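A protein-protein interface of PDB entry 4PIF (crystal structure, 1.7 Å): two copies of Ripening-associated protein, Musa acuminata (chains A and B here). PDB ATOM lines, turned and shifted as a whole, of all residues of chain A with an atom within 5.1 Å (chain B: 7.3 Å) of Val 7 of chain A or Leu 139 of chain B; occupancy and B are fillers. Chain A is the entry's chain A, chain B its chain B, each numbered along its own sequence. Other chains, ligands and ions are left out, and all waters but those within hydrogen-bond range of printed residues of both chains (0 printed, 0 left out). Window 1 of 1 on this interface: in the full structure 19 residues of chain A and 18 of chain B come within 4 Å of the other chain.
N of Leu 139 of chain A lies within hydrogen-bond range of O of Ile 5 of chain A (2.9 Å).
The backbone NH of Val 7 of chain A lies within hydrogen-bond range of the backbone carbonyl oxygen of Val 137 of chain A, at 2.9 Å.
The backbone carbonyl oxygen (O) of Phe 125 of chain A is in hydrogen-bond range of the backbone NH (N) of Gly 136 of chain A (2.7 Å).
The backbone carbonyl oxygen of Ile 5 of chain B lies within hydrogen-bond range of the backbone NH of Leu 139 of chain B, 2.9 Å away.
The backbone NH of Val 137 of chain B sits at hydrogen-bond distance from the backbone carbonyl oxygen of Val 7 of chain B.
The backbone carbonyl oxygen of Val 74 of chain B lies close to the backbone NH of Ile 116 of chain B, 3.3 Å away.
O of Lys 6 of chain A lies within hydrogen-bond range of N of Ala 117 of chain B, 2.9 Å away.
O of Ala 118 of chain B lies within hydrogen-bond range of N of Lys 6 of chain A (3.0 Å).
The backbone NH (N) of Gly 8 of chain A lies within hydrogen-bond range of the backbone carbonyl oxygen (O) of Pro 115 of chain B (2.8 Å).
Printed residues of chain B within 4 Å of Ala 9 of chain A: Pro 115.
Of the printed residues of chain A, Ile 5 of chain B touches Ile 5 (3.97 Å) and Leu 139 (3.7 Å).
Printed residues of chain A within 4 Å of Val 7 of chain B: Leu 139 (3.6 Å).
Of the printed residues of chain A, Leu 114 of chain B touches Leu 114 (3.7 Å).
Leu 139 of chain B touches just these residues of chain A: Ile 5 and Val 7.
Of the printed residues of chain A, Glu 140 of chain B touches Ile 5.
The nearest printed residue of chain B that does not touch Leu 139 of chain A is Leu 139 of chain B (4.04 Å).
Of the 11 printed residues of chain A, 9 touch a printed residue of chain B.
Of the 23 printed residues of chain B, 10 touch a printed residue of chain A.
Hydrophobic or aromatic side chains of chain B that line the printed part of chain A: Ile 5, Val 7, Leu 114, Pro 115, Ile 116, Ala 117, Ala 118, Leu 139 and Pro 141.
Ile 5 of chain B touches its own counterpart, Ile 5 of chain A.
Ile 5 of chain A touches Leu 139 of chain B, and with the chains exchanged Leu 139 of chain A touches Ile 5 of chain B.
Val 7 of chain A touches Leu 139 of chain B, and with the chains exchanged Leu 139 of chain A touches Val 7 of chain B.
Leu 114 of chain A touches its own counterpart, Leu 114 of chain B.
Of the 18 pairs that touch across the chains among the printed residues, 6 have their exchanged pair printed and touching as well.
Among the printed residues, pairs that only touch across the chains: Ile 5 of chain A with Glu 140 of chain B (3.2 Å), Ile 5 of chain A with Pro 141 of chain B (3.4 Å), Ile 5 of chain A with Ala 118 of chain B (3.5 Å), Val 7 of chain A with Pro 115 of chain B (3.6 Å), Gly 8 of chain A with Ala 117 of chain B (3.6 Å), Leu 139 of chain A with Val 7 of chain B (3.6 Å), Lys 6 of chain A with Ile 116 of chain B (3.6 Å), Trp 10 of chain A with Pro 115 of chain B (3.6 Å), Leu 139 of chain A with Ile 5 of chain B (3.7 Å), Leu 114 of chain A with Leu 114 of chain B (3.7 Å), Val 7 of chain A with Leu 139 of chain B (3.7 Å), Ile 5 of chain A with Leu 139 of chain B (3.9 Å), Phe 125 of chain A with Ala 117 of chain B (3.9 Å), Ala 9 of chain A with Pro 115 of chain B (3.96 Å) and Ile 5 of chain A with Ile 5 of chain B (3.97 Å).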
ATOM      1  N   ILE A   5     -35.198 -15.151   8.574  1.00  0.00           N
ATOM      2  CA  ILE A   5     -34.068 -14.295   8.197  1.00  0.00           C
ATOM      3  C   ILE A   5     -34.496 -13.524   6.967  1.00  0.00           C
ATOM      4  O   ILE A   5     -34.818 -14.136   5.956  1.00  0.00           O
ATOM      5  CB  ILE A   5     -32.784 -15.121   7.883  1.00  0.00           C
ATOM      6  CG1 ILE A   5     -32.343 -15.996   9.081  1.00  0.00           C
ATOM      7  CG2 ILE A   5     -31.673 -14.197   7.370  1.00  0.00           C
ATOM      8  CD1 ILE A   5     -31.954 -15.213  10.273  1.00  0.00           C
ATOM      9  N   LYS A   6     -34.487 -12.195   7.049  1.00  0.00           N
ATOM     10  CA  LYS A   6     -34.895 -11.334   5.940  1.00  0.00           C
ATOM     11  C   LYS A   6     -33.795 -10.296   5.773  1.00  0.00           C
ATOM     12  O   LYS A   6     -33.483  -9.551   6.709  1.00  0.00           O
ATOM     13  CB  LYS A   6     -36.204 -10.621   6.279  1.00  0.00           C
ATOM     14  CG  LYS A   6     -37.404 -11.563   6.403  1.00  0.00           C
ATOM     15  CD  LYS A   6     -38.691 -10.841   6.847  1.00  0.00           C
ATOM     16  CE  LYS A   6     -39.219  -9.817   5.858  1.00  0.00           C
ATOM     17  NZ  LYS A   6     -40.531  -9.252   6.336  1.00  0.00           N
ATOM     18  N   VAL A   7     -33.185 -10.275   4.601  1.00  0.00           N
ATOM     19  CA  VAL A   7     -32.114  -9.311   4.295  1.00  0.00           C
ATOM     20  C   VAL A   7     -32.571  -8.396   3.184  1.00  0.00           C
ATOM     21  O   VAL A   7     -33.325  -8.820   2.314  1.00  0.00           O
ATOM     22  CB  VAL A   7     -30.743  -9.954   4.036  1.00  0.00           C
ATOM     23  CG1 VAL A   7     -30.283 -10.750   5.264  1.00  0.00           C
ATOM     24  CG2 VAL A   7     -30.777 -10.842   2.797  1.00  0.00           C
ATOM     25  N   GLY A   8     -32.104  -7.160   3.215  1.00  0.00           N
ATOM     26  CA  GLY A   8     -32.643  -6.106   2.366  1.00  0.00           C
ATOM     27  C   GLY A   8     -33.721  -5.377   3.169  1.00  0.00           C
ATOM     28  O   GLY A   8     -33.744  -5.493   4.400  1.00  0.00           O
ATOM     29  N   ALA A   9     -34.630  -4.605   2.531  1.00  0.00           N
ATOM     30  CA  ALA A   9     -34.673  -4.452   1.075  1.00  0.00           C
ATOM     31  C   ALA A   9     -33.669  -3.439   0.588  1.00  0.00           C
ATOM     32  O   ALA A   9     -33.241  -2.553   1.358  1.00  0.00           O
ATOM     33  CB  ALA A   9     -36.072  -4.015   0.647  1.00  0.00           C
ATOM     34  N   TRP A  10     -33.309  -3.563  -0.699  1.00  0.00           N
ATOM     35  CA  TRP A  10     -32.479  -2.606  -1.415  1.00  0.00           C
ATOM     36  C   TRP A  10     -33.433  -1.896  -2.356  1.00  0.00           C
ATOM     37  O   TRP A  10     -34.248  -2.546  -3.016  1.00  0.00           O
ATOM     38  CB  TRP A  10     -31.365  -3.307  -2.265  1.00  0.00           C
ATOM     39  CG  TRP A  10     -30.299  -3.950  -1.425  1.00  0.00           C
ATOM     40  CD1 TRP A  10     -29.163  -3.361  -0.946  1.00  0.00           C
ATOM     41  CD2 TRP A  10     -30.289  -5.302  -0.942  1.00  0.00           C
ATOM     42  NE1 TRP A  10     -28.444  -4.264  -0.196  1.00  0.00           N
ATOM     43  CE2 TRP A  10     -29.111  -5.462  -0.171  1.00  0.00           C
ATOM     44  CE3 TRP A  10     -31.190  -6.388  -1.053  1.00  0.00           C
ATOM     45  CZ2 TRP A  10     -28.768  -6.680   0.440  1.00  0.00           C
ATOM     46  CZ3 TRP A  10     -30.867  -7.593  -0.422  1.00  0.00           C
ATOM     47  CH2 TRP A  10     -29.683  -7.721   0.338  1.00  0.00           C
ATOM     48  N   LEU A 114     -25.611  -9.751  -3.106  1.00  0.00           N
ATOM     49  CA  LEU A 114     -25.839 -10.676  -2.020  1.00  0.00           C
ATOM     50  C   LEU A 114     -25.389 -12.093  -2.399  1.00  0.00           C
ATOM     51  O   LEU A 114     -26.205 -12.917  -2.828  1.00  0.00           O
ATOM     52  CB  LEU A 114     -27.306 -10.654  -1.533  1.00  0.00           C
ATOM     53  CG  LEU A 114     -27.582 -11.542  -0.311  1.00  0.00           C
ATOM     54  CD1 LEU A 114     -27.150 -10.866   0.978  1.00  0.00           C
ATOM     55  CD2 LEU A 114     -29.050 -11.920  -0.227  1.00  0.00           C
ATOM     56  N   PHE A 125     -39.632  -9.925  -0.414  1.00  0.00           N
ATOM     57  CA  PHE A 125     -40.412  -8.835   0.168  1.00  0.00           C
ATOM     58  C   PHE A 125     -39.855  -7.555  -0.450  1.00  0.00           C
ATOM     59  O   PHE A 125     -38.807  -7.597  -1.115  1.00  0.00           O
ATOM     60  CB  PHE A 125     -40.346  -8.808   1.706  1.00  0.00           C
ATOM     61  CG  PHE A 125     -38.987  -8.494   2.271  1.00  0.00           C
ATOM     62  CD1 PHE A 125     -38.034  -9.499   2.430  1.00  0.00           C
ATOM     63  CD2 PHE A 125     -38.670  -7.203   2.679  1.00  0.00           C
ATOM     64  CE1 PHE A 125     -36.771  -9.206   2.966  1.00  0.00           C
ATOM     65  CE2 PHE A 125     -37.409  -6.909   3.209  1.00  0.00           C
ATOM     66  CZ  PHE A 125     -36.468  -7.916   3.339  1.00  0.00           C
ATOM     67  N   GLY A 136     -36.081  -7.403  -1.228  1.00  0.00           N
ATOM     68  CA  GLY A 136     -35.290  -8.108  -0.234  1.00  0.00           C
ATOM     69  C   GLY A 136     -35.640  -9.575  -0.331  1.00  0.00           C
ATOM     70  O   GLY A 136     -36.566  -9.964  -1.066  1.00  0.00           O
ATOM     71  N   VAL A 137     -34.914 -10.404   0.422  1.00  0.00           N
ATOM     72  CA  VAL A 137     -35.132 -11.838   0.383  1.00  0.00           C
ATOM     73  C   VAL A 137     -35.190 -12.475   1.745  1.00  0.00           C
ATOM     74  O   VAL A 137     -34.545 -12.010   2.698  1.00  0.00           O
ATOM     75  CB  VAL A 137     -34.033 -12.552  -0.457  1.00  0.00           C
ATOM     76  CG1 VAL A 137     -34.122 -12.184  -1.929  1.00  0.00           C
ATOM     77  CG2 VAL A 137     -32.636 -12.257   0.091  1.00  0.00           C
ATOM     78  N   LEU A 139     -34.048 -15.833   3.686  1.00  0.00           N
ATOM     79  CA  LEU A 139     -32.993 -16.837   3.557  1.00  0.00           C
ATOM     80  C   LEU A 139     -33.299 -18.040   4.398  1.00  0.00           C
ATOM     81  O   LEU A 139     -33.798 -17.907   5.519  1.00  0.00           O
ATOM     82  CB  LEU A 139     -31.611 -16.297   3.985  1.00  0.00           C
ATOM     83  CG  LEU A 139     -31.132 -15.077   3.181  1.00  0.00           C
ATOM     84  CD1 LEU A 139     -29.808 -14.564   3.716  1.00  0.00           C
ATOM     85  CD2 LEU A 139     -31.044 -15.411   1.664  1.00  0.00           C
ATOM     86  N   GLY B   3     -27.225 -25.982   9.862  1.00  0.00           N
ATOM     87  CA  GLY B   3     -28.215 -24.979   9.535  1.00  0.00           C
ATOM     88  C   GLY B   3     -27.691 -23.566   9.482  1.00  0.00           C
ATOM     89  O   GLY B   3     -28.483 -22.632   9.505  1.00  0.00           O
ATOM     90  N   ALA B   4     -26.372 -23.417   9.295  1.00  0.00           N
ATOM     91  CA  ALA B   4     -25.788 -22.083   9.197  1.00  0.00           C
ATOM     92  C   ALA B   4     -26.269 -21.367   7.957  1.00  0.00           C
ATOM     93  O   ALA B   4     -26.527 -22.004   6.915  1.00  0.00           O
ATOM     94  CB  ALA B   4     -24.275 -22.203   9.126  1.00  0.00           C
ATOM     95  N   ILE B   5     -26.385 -20.035   8.068  1.00  0.00           N
ATOM     96  CA  ILE B   5     -26.644 -19.145   6.935  1.00  0.00           C
ATOM     97  C   ILE B   5     -25.441 -18.183   6.886  1.00  0.00           C
ATOM     98  O   ILE B   5     -25.210 -17.447   7.855  1.00  0.00           O
ATOM     99  CB  ILE B   5     -27.996 -18.395   6.987  1.00  0.00           C
ATOM    100  CG1 ILE B   5     -29.159 -19.415   6.793  1.00  0.00           C
ATOM    101  CG2 ILE B   5     -28.033 -17.321   5.870  1.00  0.00           C
ATOM    102  CD1 ILE B   5     -30.555 -18.834   6.965  1.00  0.00           C
ATOM    103  N   LYS B   6     -24.713 -18.188   5.758  1.00  0.00           N
ATOM    104  CA  LYS B   6     -23.515 -17.322   5.567  1.00  0.00           C
ATOM    105  C   LYS B   6     -23.745 -16.480   4.322  1.00  0.00           C
ATOM    106  O   LYS B   6     -24.059 -17.022   3.259  1.00  0.00           O
ATOM    107  CB  LYS B   6     -22.252 -18.184   5.349  1.00  0.00           C
ATOM    108  CG  LYS B   6     -21.892 -19.025   6.592  1.00  0.00           C
ATOM    109  CD  LYS B   6     -20.796 -20.078   6.282  1.00  0.00           C
ATOM    110  CE  LYS B   6     -19.410 -19.491   6.100  1.00  0.00           C
ATOM    111  NZ  LYS B   6     -18.397 -20.541   5.799  1.00  0.00           N
ATOM    112  N   VAL B   7     -23.607 -15.160   4.463  1.00  0.00           N
ATOM    113  CA  VAL B   7     -23.741 -14.234   3.336  1.00  0.00           C
ATOM    114  C   VAL B   7     -22.415 -13.491   3.169  1.00  0.00           C
ATOM    115  O   VAL B   7     -21.742 -13.192   4.160  1.00  0.00           O
ATOM    116  CB  VAL B   7     -24.978 -13.295   3.377  1.00  0.00           C
ATOM    117  CG1 VAL B   7     -26.279 -14.128   3.424  1.00  0.00           C
ATOM    118  CG2 VAL B   7     -24.936 -12.353   4.567  1.00  0.00           C
ATOM    119  N   PRO B  22     -20.153 -19.701  13.834  1.00  0.00           N
ATOM    120  CA  PRO B  22     -21.253 -18.974  14.490  1.00  0.00           C
ATOM    121  C   PRO B  22     -21.504 -19.344  15.949  1.00  0.00           C
ATOM    122  O   PRO B  22     -22.572 -19.013  16.456  1.00  0.00           O
ATOM    123  CB  PRO B  22     -22.457 -19.489  13.699  1.00  0.00           C
ATOM    124  CG  PRO B  22     -22.107 -20.934  13.447  1.00  0.00           C
ATOM    125  CD  PRO B  22     -20.590 -21.046  13.406  1.00  0.00           C
ATOM    126  N   LEU B  73     -25.599  -6.775  16.358  1.00  0.00           N
ATOM    127  CA  LEU B  73     -25.239  -6.244  15.038  1.00  0.00           C
ATOM    128  C   LEU B  73     -26.336  -6.589  14.056  1.00  0.00           C
ATOM    129  O   LEU B  73     -26.694  -7.770  13.932  1.00  0.00           O
ATOM    130  CB  LEU B  73     -23.898  -6.798  14.562  1.00  0.00           C
ATOM    131  CG  LEU B  73     -22.669  -6.449  15.445  1.00  0.00           C
ATOM    132  CD1 LEU B  73     -21.544  -7.491  15.242  1.00  0.00           C
ATOM    133  CD2 LEU B  73     -22.174  -5.006  15.171  1.00  0.00           C
ATOM    134  N   VAL B  74     -26.899  -5.575  13.390  1.00  0.00           N
ATOM    135  CA  VAL B  74     -28.029  -5.750  12.473  1.00  0.00           C
ATOM    136  C   VAL B  74     -27.780  -5.225  11.066  1.00  0.00           C
ATOM    137  O   VAL B  74     -28.690  -5.222  10.258  1.00  0.00           O
ATOM    138  CB  VAL B  74     -29.343  -5.172  13.049  1.00  0.00           C
ATOM    139  CG1 VAL B  74     -29.696  -5.857  14.351  1.00  0.00           C
ATOM    140  CG2 VAL B  74     -29.278  -3.642  13.208  1.00  0.00           C
ATOM    141  N   LEU B 114     -25.554  -4.525   3.575  1.00  0.00           N
ATOM    142  CA  LEU B 114     -26.333  -5.609   4.114  1.00  0.00           C
ATOM    143  C   LEU B 114     -27.303  -5.103   5.172  1.00  0.00           C
ATOM    144  O   LEU B 114     -27.024  -5.194   6.370  1.00  0.00           O
ATOM    145  CB  LEU B 114     -25.455  -6.800   4.602  1.00  0.00           C
ATOM    146  CG  LEU B 114     -26.203  -8.012   5.162  1.00  0.00           C
ATOM    147  CD1 LEU B 114     -26.853  -8.859   4.045  1.00  0.00           C
ATOM    148  CD2 LEU B 114     -25.284  -8.866   5.989  1.00  0.00           C
ATOM    149  N   PRO B 115     -28.456  -4.539   4.760  1.00  0.00           N
ATOM    150  CA  PRO B 115     -29.488  -4.202   5.763  1.00  0.00           C
ATOM    151  C   PRO B 115     -30.196  -5.506   6.163  1.00  0.00           C
ATOM    152  O   PRO B 115     -30.377  -6.376   5.309  1.00  0.00           O
ATOM    153  CB  PRO B 115     -30.422  -3.242   5.014  1.00  0.00           C
ATOM    154  CG  PRO B 115     -30.072  -3.335   3.595  1.00  0.00           C
ATOM    155  CD  PRO B 115     -28.969  -4.346   3.387  1.00  0.00           C
ATOM    156  N   ILE B 116     -30.453  -5.719   7.468  1.00  0.00           N
ATOM    157  CA  ILE B 116     -31.053  -6.990   7.930  1.00  0.00           C
ATOM    158  C   ILE B 116     -32.392  -6.640   8.520  1.00  0.00           C
ATOM    159  O   ILE B 116     -32.452  -6.110   9.639  1.00  0.00           O
ATOM    160  CB  ILE B 116     -30.180  -7.807   8.935  1.00  0.00           C
ATOM    161  CG1 ILE B 116     -28.743  -8.039   8.393  1.00  0.00           C
ATOM    162  CG2 ILE B 116     -30.862  -9.181   9.241  1.00  0.00           C
ATOM    163  CD1 ILE B 116     -27.740  -8.578   9.401  1.00  0.00           C
ATOM    164  N   ALA B 117     -33.458  -6.886   7.758  1.00  0.00           N
ATOM    165  CA  ALA B 117     -34.818  -6.580   8.196  1.00  0.00           C
ATOM    166  C   ALA B 117     -35.251  -7.465   9.365  1.00  0.00           C
ATOM    167  O   ALA B 117     -36.004  -7.021  10.232  1.00  0.00           O
ATOM    168  CB  ALA B 117     -35.794  -6.724   7.040  1.00  0.00           C
ATOM    169  N   ALA B 118     -34.823  -8.726   9.367  1.00  0.00           N
ATOM    170  CA  ALA B 118     -35.137  -9.640  10.465  1.00  0.00           C
ATOM    171  C   ALA B 118     -33.939 -10.548  10.637  1.00  0.00           C
ATOM    172  O   ALA B 118     -33.523 -11.225   9.703  1.00  0.00           O
ATOM    173  CB  ALA B 118     -36.404 -10.440  10.151  1.00  0.00           C
ATOM    174  N   GLY B 119     -33.292 -10.440  11.786  1.00  0.00           N
ATOM    175  CA  GLY B 119     -32.119 -11.252  12.054  1.00  0.00           C
ATOM    176  C   GLY B 119     -30.966 -10.420  12.577  1.00  0.00           C
ATOM    177  O   GLY B 119     -31.070  -9.198  12.693  1.00  0.00           O
ATOM    178  N   LYS B 120     -29.854 -11.086  12.863  1.00  0.00           N
ATOM    179  CA  LYS B 120     -28.669 -10.410  13.377  1.00  0.00           C
ATOM    180  C   LYS B 120     -27.431 -11.172  12.954  1.00  0.00           C
ATOM    181  O   LYS B 120     -27.518 -12.340  12.548  1.00  0.00           O
ATOM    182  CB  LYS B 120     -28.731 -10.315  14.922  1.00  0.00           C
ATOM    183  CG  LYS B 120     -28.683 -11.683  15.623  1.00  0.00           C
ATOM    184  CD  LYS B 120     -28.642 -11.421  17.112  1.00  0.00           C
ATOM    185  CE  LYS B 120     -28.832 -12.723  17.853  1.00  0.00           C
ATOM    186  NZ  LYS B 120     -27.657 -13.032  18.702  1.00  0.00           N
ATOM    187  N   ILE B 121     -26.280 -10.494  13.019  1.00  0.00           N
ATOM    188  CA  ILE B 121     -24.996 -11.107  12.701  1.00  0.00           C
ATOM    189  C   ILE B 121     -24.547 -11.928  13.908  1.00  0.00           C
ATOM    190  O   ILE B 121     -24.542 -11.417  15.038  1.00  0.00           O
ATOM    191  CB  ILE B 121     -23.979  -9.998  12.353  1.00  0.00           C
ATOM    192  CG1 ILE B 121     -24.364  -9.370  10.959  1.00  0.00           C
ATOM    193  CG2 ILE B 121     -22.527 -10.574  12.371  1.00  0.00           C
ATOM    194  CD1 ILE B 121     -23.720  -7.997  10.694  1.00  0.00           C
ATOM    195  N   SER B 122     -24.144 -13.191  13.669  1.00  0.00           N
ATOM    196  CA  SER B 122     -23.697 -14.103  14.731  1.00  0.00           C
ATOM    197  C   SER B 122     -22.249 -14.604  14.604  1.00  0.00           C
ATOM    198  O   SER B 122     -21.770 -15.322  15.482  1.00  0.00           O
ATOM    199  CB  SER B 122     -24.632 -15.303  14.812  1.00  0.00           C
ATOM    200  OG  SER B 122     -24.583 -15.979  13.568  1.00  0.00           O
ATOM    201  N   GLY B 123     -21.553 -14.211  13.543  1.00  0.00           N
ATOM    202  CA  GLY B 123     -20.169 -14.579  13.375  1.00  0.00           C
ATOM    203  C   GLY B 123     -19.644 -14.014  12.089  1.00  0.00           C
ATOM    204  O   GLY B 123     -20.406 -13.412  11.312  1.00  0.00           O
ATOM    205  N   VAL B 137     -20.590 -12.679   6.818  1.00  0.00           N
ATOM    206  CA  VAL B 137     -21.197 -12.866   8.135  1.00  0.00           C
ATOM    207  C   VAL B 137     -22.106 -14.074   8.177  1.00  0.00           C
ATOM    208  O   VAL B 137     -22.702 -14.449   7.172  1.00  0.00           O
ATOM    209  CB  VAL B 137     -22.010 -11.631   8.622  1.00  0.00           C
ATOM    210  CG1 VAL B 137     -21.105 -10.415   8.876  1.00  0.00           C
ATOM    211  CG2 VAL B 137     -23.126 -11.266   7.641  1.00  0.00           C
ATOM    212  N   TYR B 138     -22.214 -14.650   9.360  1.00  0.00           N
ATOM    213  CA  TYR B 138     -23.201 -15.684   9.665  1.00  0.00           C
ATOM    214  C   TYR B 138     -24.410 -14.935  10.183  1.00  0.00           C
ATOM    215  O   TYR B 138     -24.258 -13.895  10.850  1.00  0.00           O
ATOM    216  CB  TYR B 138     -22.728 -16.597  10.805  1.00  0.00           C
ATOM    217  CG  TYR B 138     -21.699 -17.604  10.388  1.00  0.00           C
ATOM    218  CD1 TYR B 138     -20.357 -17.248  10.267  1.00  0.00           C
ATOM    219  CD2 TYR B 138     -22.048 -18.938  10.177  1.00  0.00           C
ATOM    220  CE1 TYR B 138     -19.389 -18.188   9.904  1.00  0.00           C
ATOM    221  CE2 TYR B 138     -21.096 -19.887   9.823  1.00  0.00           C
ATOM    222  CZ  TYR B 138     -19.765 -19.502   9.675  1.00  0.00           C
ATOM    223  OH  TYR B 138     -18.820 -20.415   9.294  1.00  0.00           O
ATOM    224  N   LEU B 139     -25.616 -15.461   9.902  1.00  0.00           N
ATOM    225  CA  LEU B 139     -26.835 -14.802  10.375  1.00  0.00           C
ATOM    226  C   LEU B 139     -27.668 -15.722  11.229  1.00  0.00           C
ATOM    227  O   LEU B 139     -27.639 -16.934  11.058  1.00  0.00           O
ATOM    228  CB  LEU B 139     -27.717 -14.351   9.198  1.00  0.00           C
ATOM    229  CG  LEU B 139     -27.060 -13.367   8.197  1.00  0.00           C
ATOM    230  CD1 LEU B 139     -27.979 -13.125   7.013  1.00  0.00           C
ATOM    231  CD2 LEU B 139     -26.731 -12.058   8.864  1.00  0.00           C
ATOM    232  N   GLU B 140     -28.449 -15.130  12.124  1.00  0.00           N
ATOM    233  CA  GLU B 140     -29.412 -15.935  12.886  1.00  0.00           C
ATOM    234  C   GLU B 140     -30.630 -15.066  13.222  1.00  0.00           C
ATOM    235  O   GLU B 140     -30.565 -13.848  13.096  1.00  0.00           O
ATOM    236  CB  GLU B 140     -28.755 -16.568  14.124  1.00  0.00           C
ATOM    237  CG  GLU B 140     -28.570 -15.665  15.311  1.00  0.00           C
ATOM    238  CD  GLU B 140     -28.209 -16.482  16.546  1.00  0.00           C
ATOM    239  OE1 GLU B 140     -27.276 -17.312  16.469  1.00  0.00           O
ATOM    240  OE2 GLU B 140     -28.959 -16.397  17.537  1.00  0.00           O
ATOM    241  N   PRO B 141     -31.778 -15.643  13.595  1.00  0.00           N
ATOM    242  CA  PRO B 141     -32.943 -14.801  13.875  1.00  0.00           C
ATOM    243  C   PRO B 141     -32.752 -13.855  15.052  1.00  0.00           C
ATOM    244  O   PRO B 141     -31.901 -14.105  15.924  1.00  0.00           O
ATOM    245  CB  PRO B 141     -34.048 -15.824  14.173  1.00  0.00           C
ATOM    246  CG  PRO B 141     -33.610 -17.061  13.485  1.00  0.00           C
ATOM    247  CD  PRO B 141     -32.124 -17.073  13.724  1.00  0.00           C
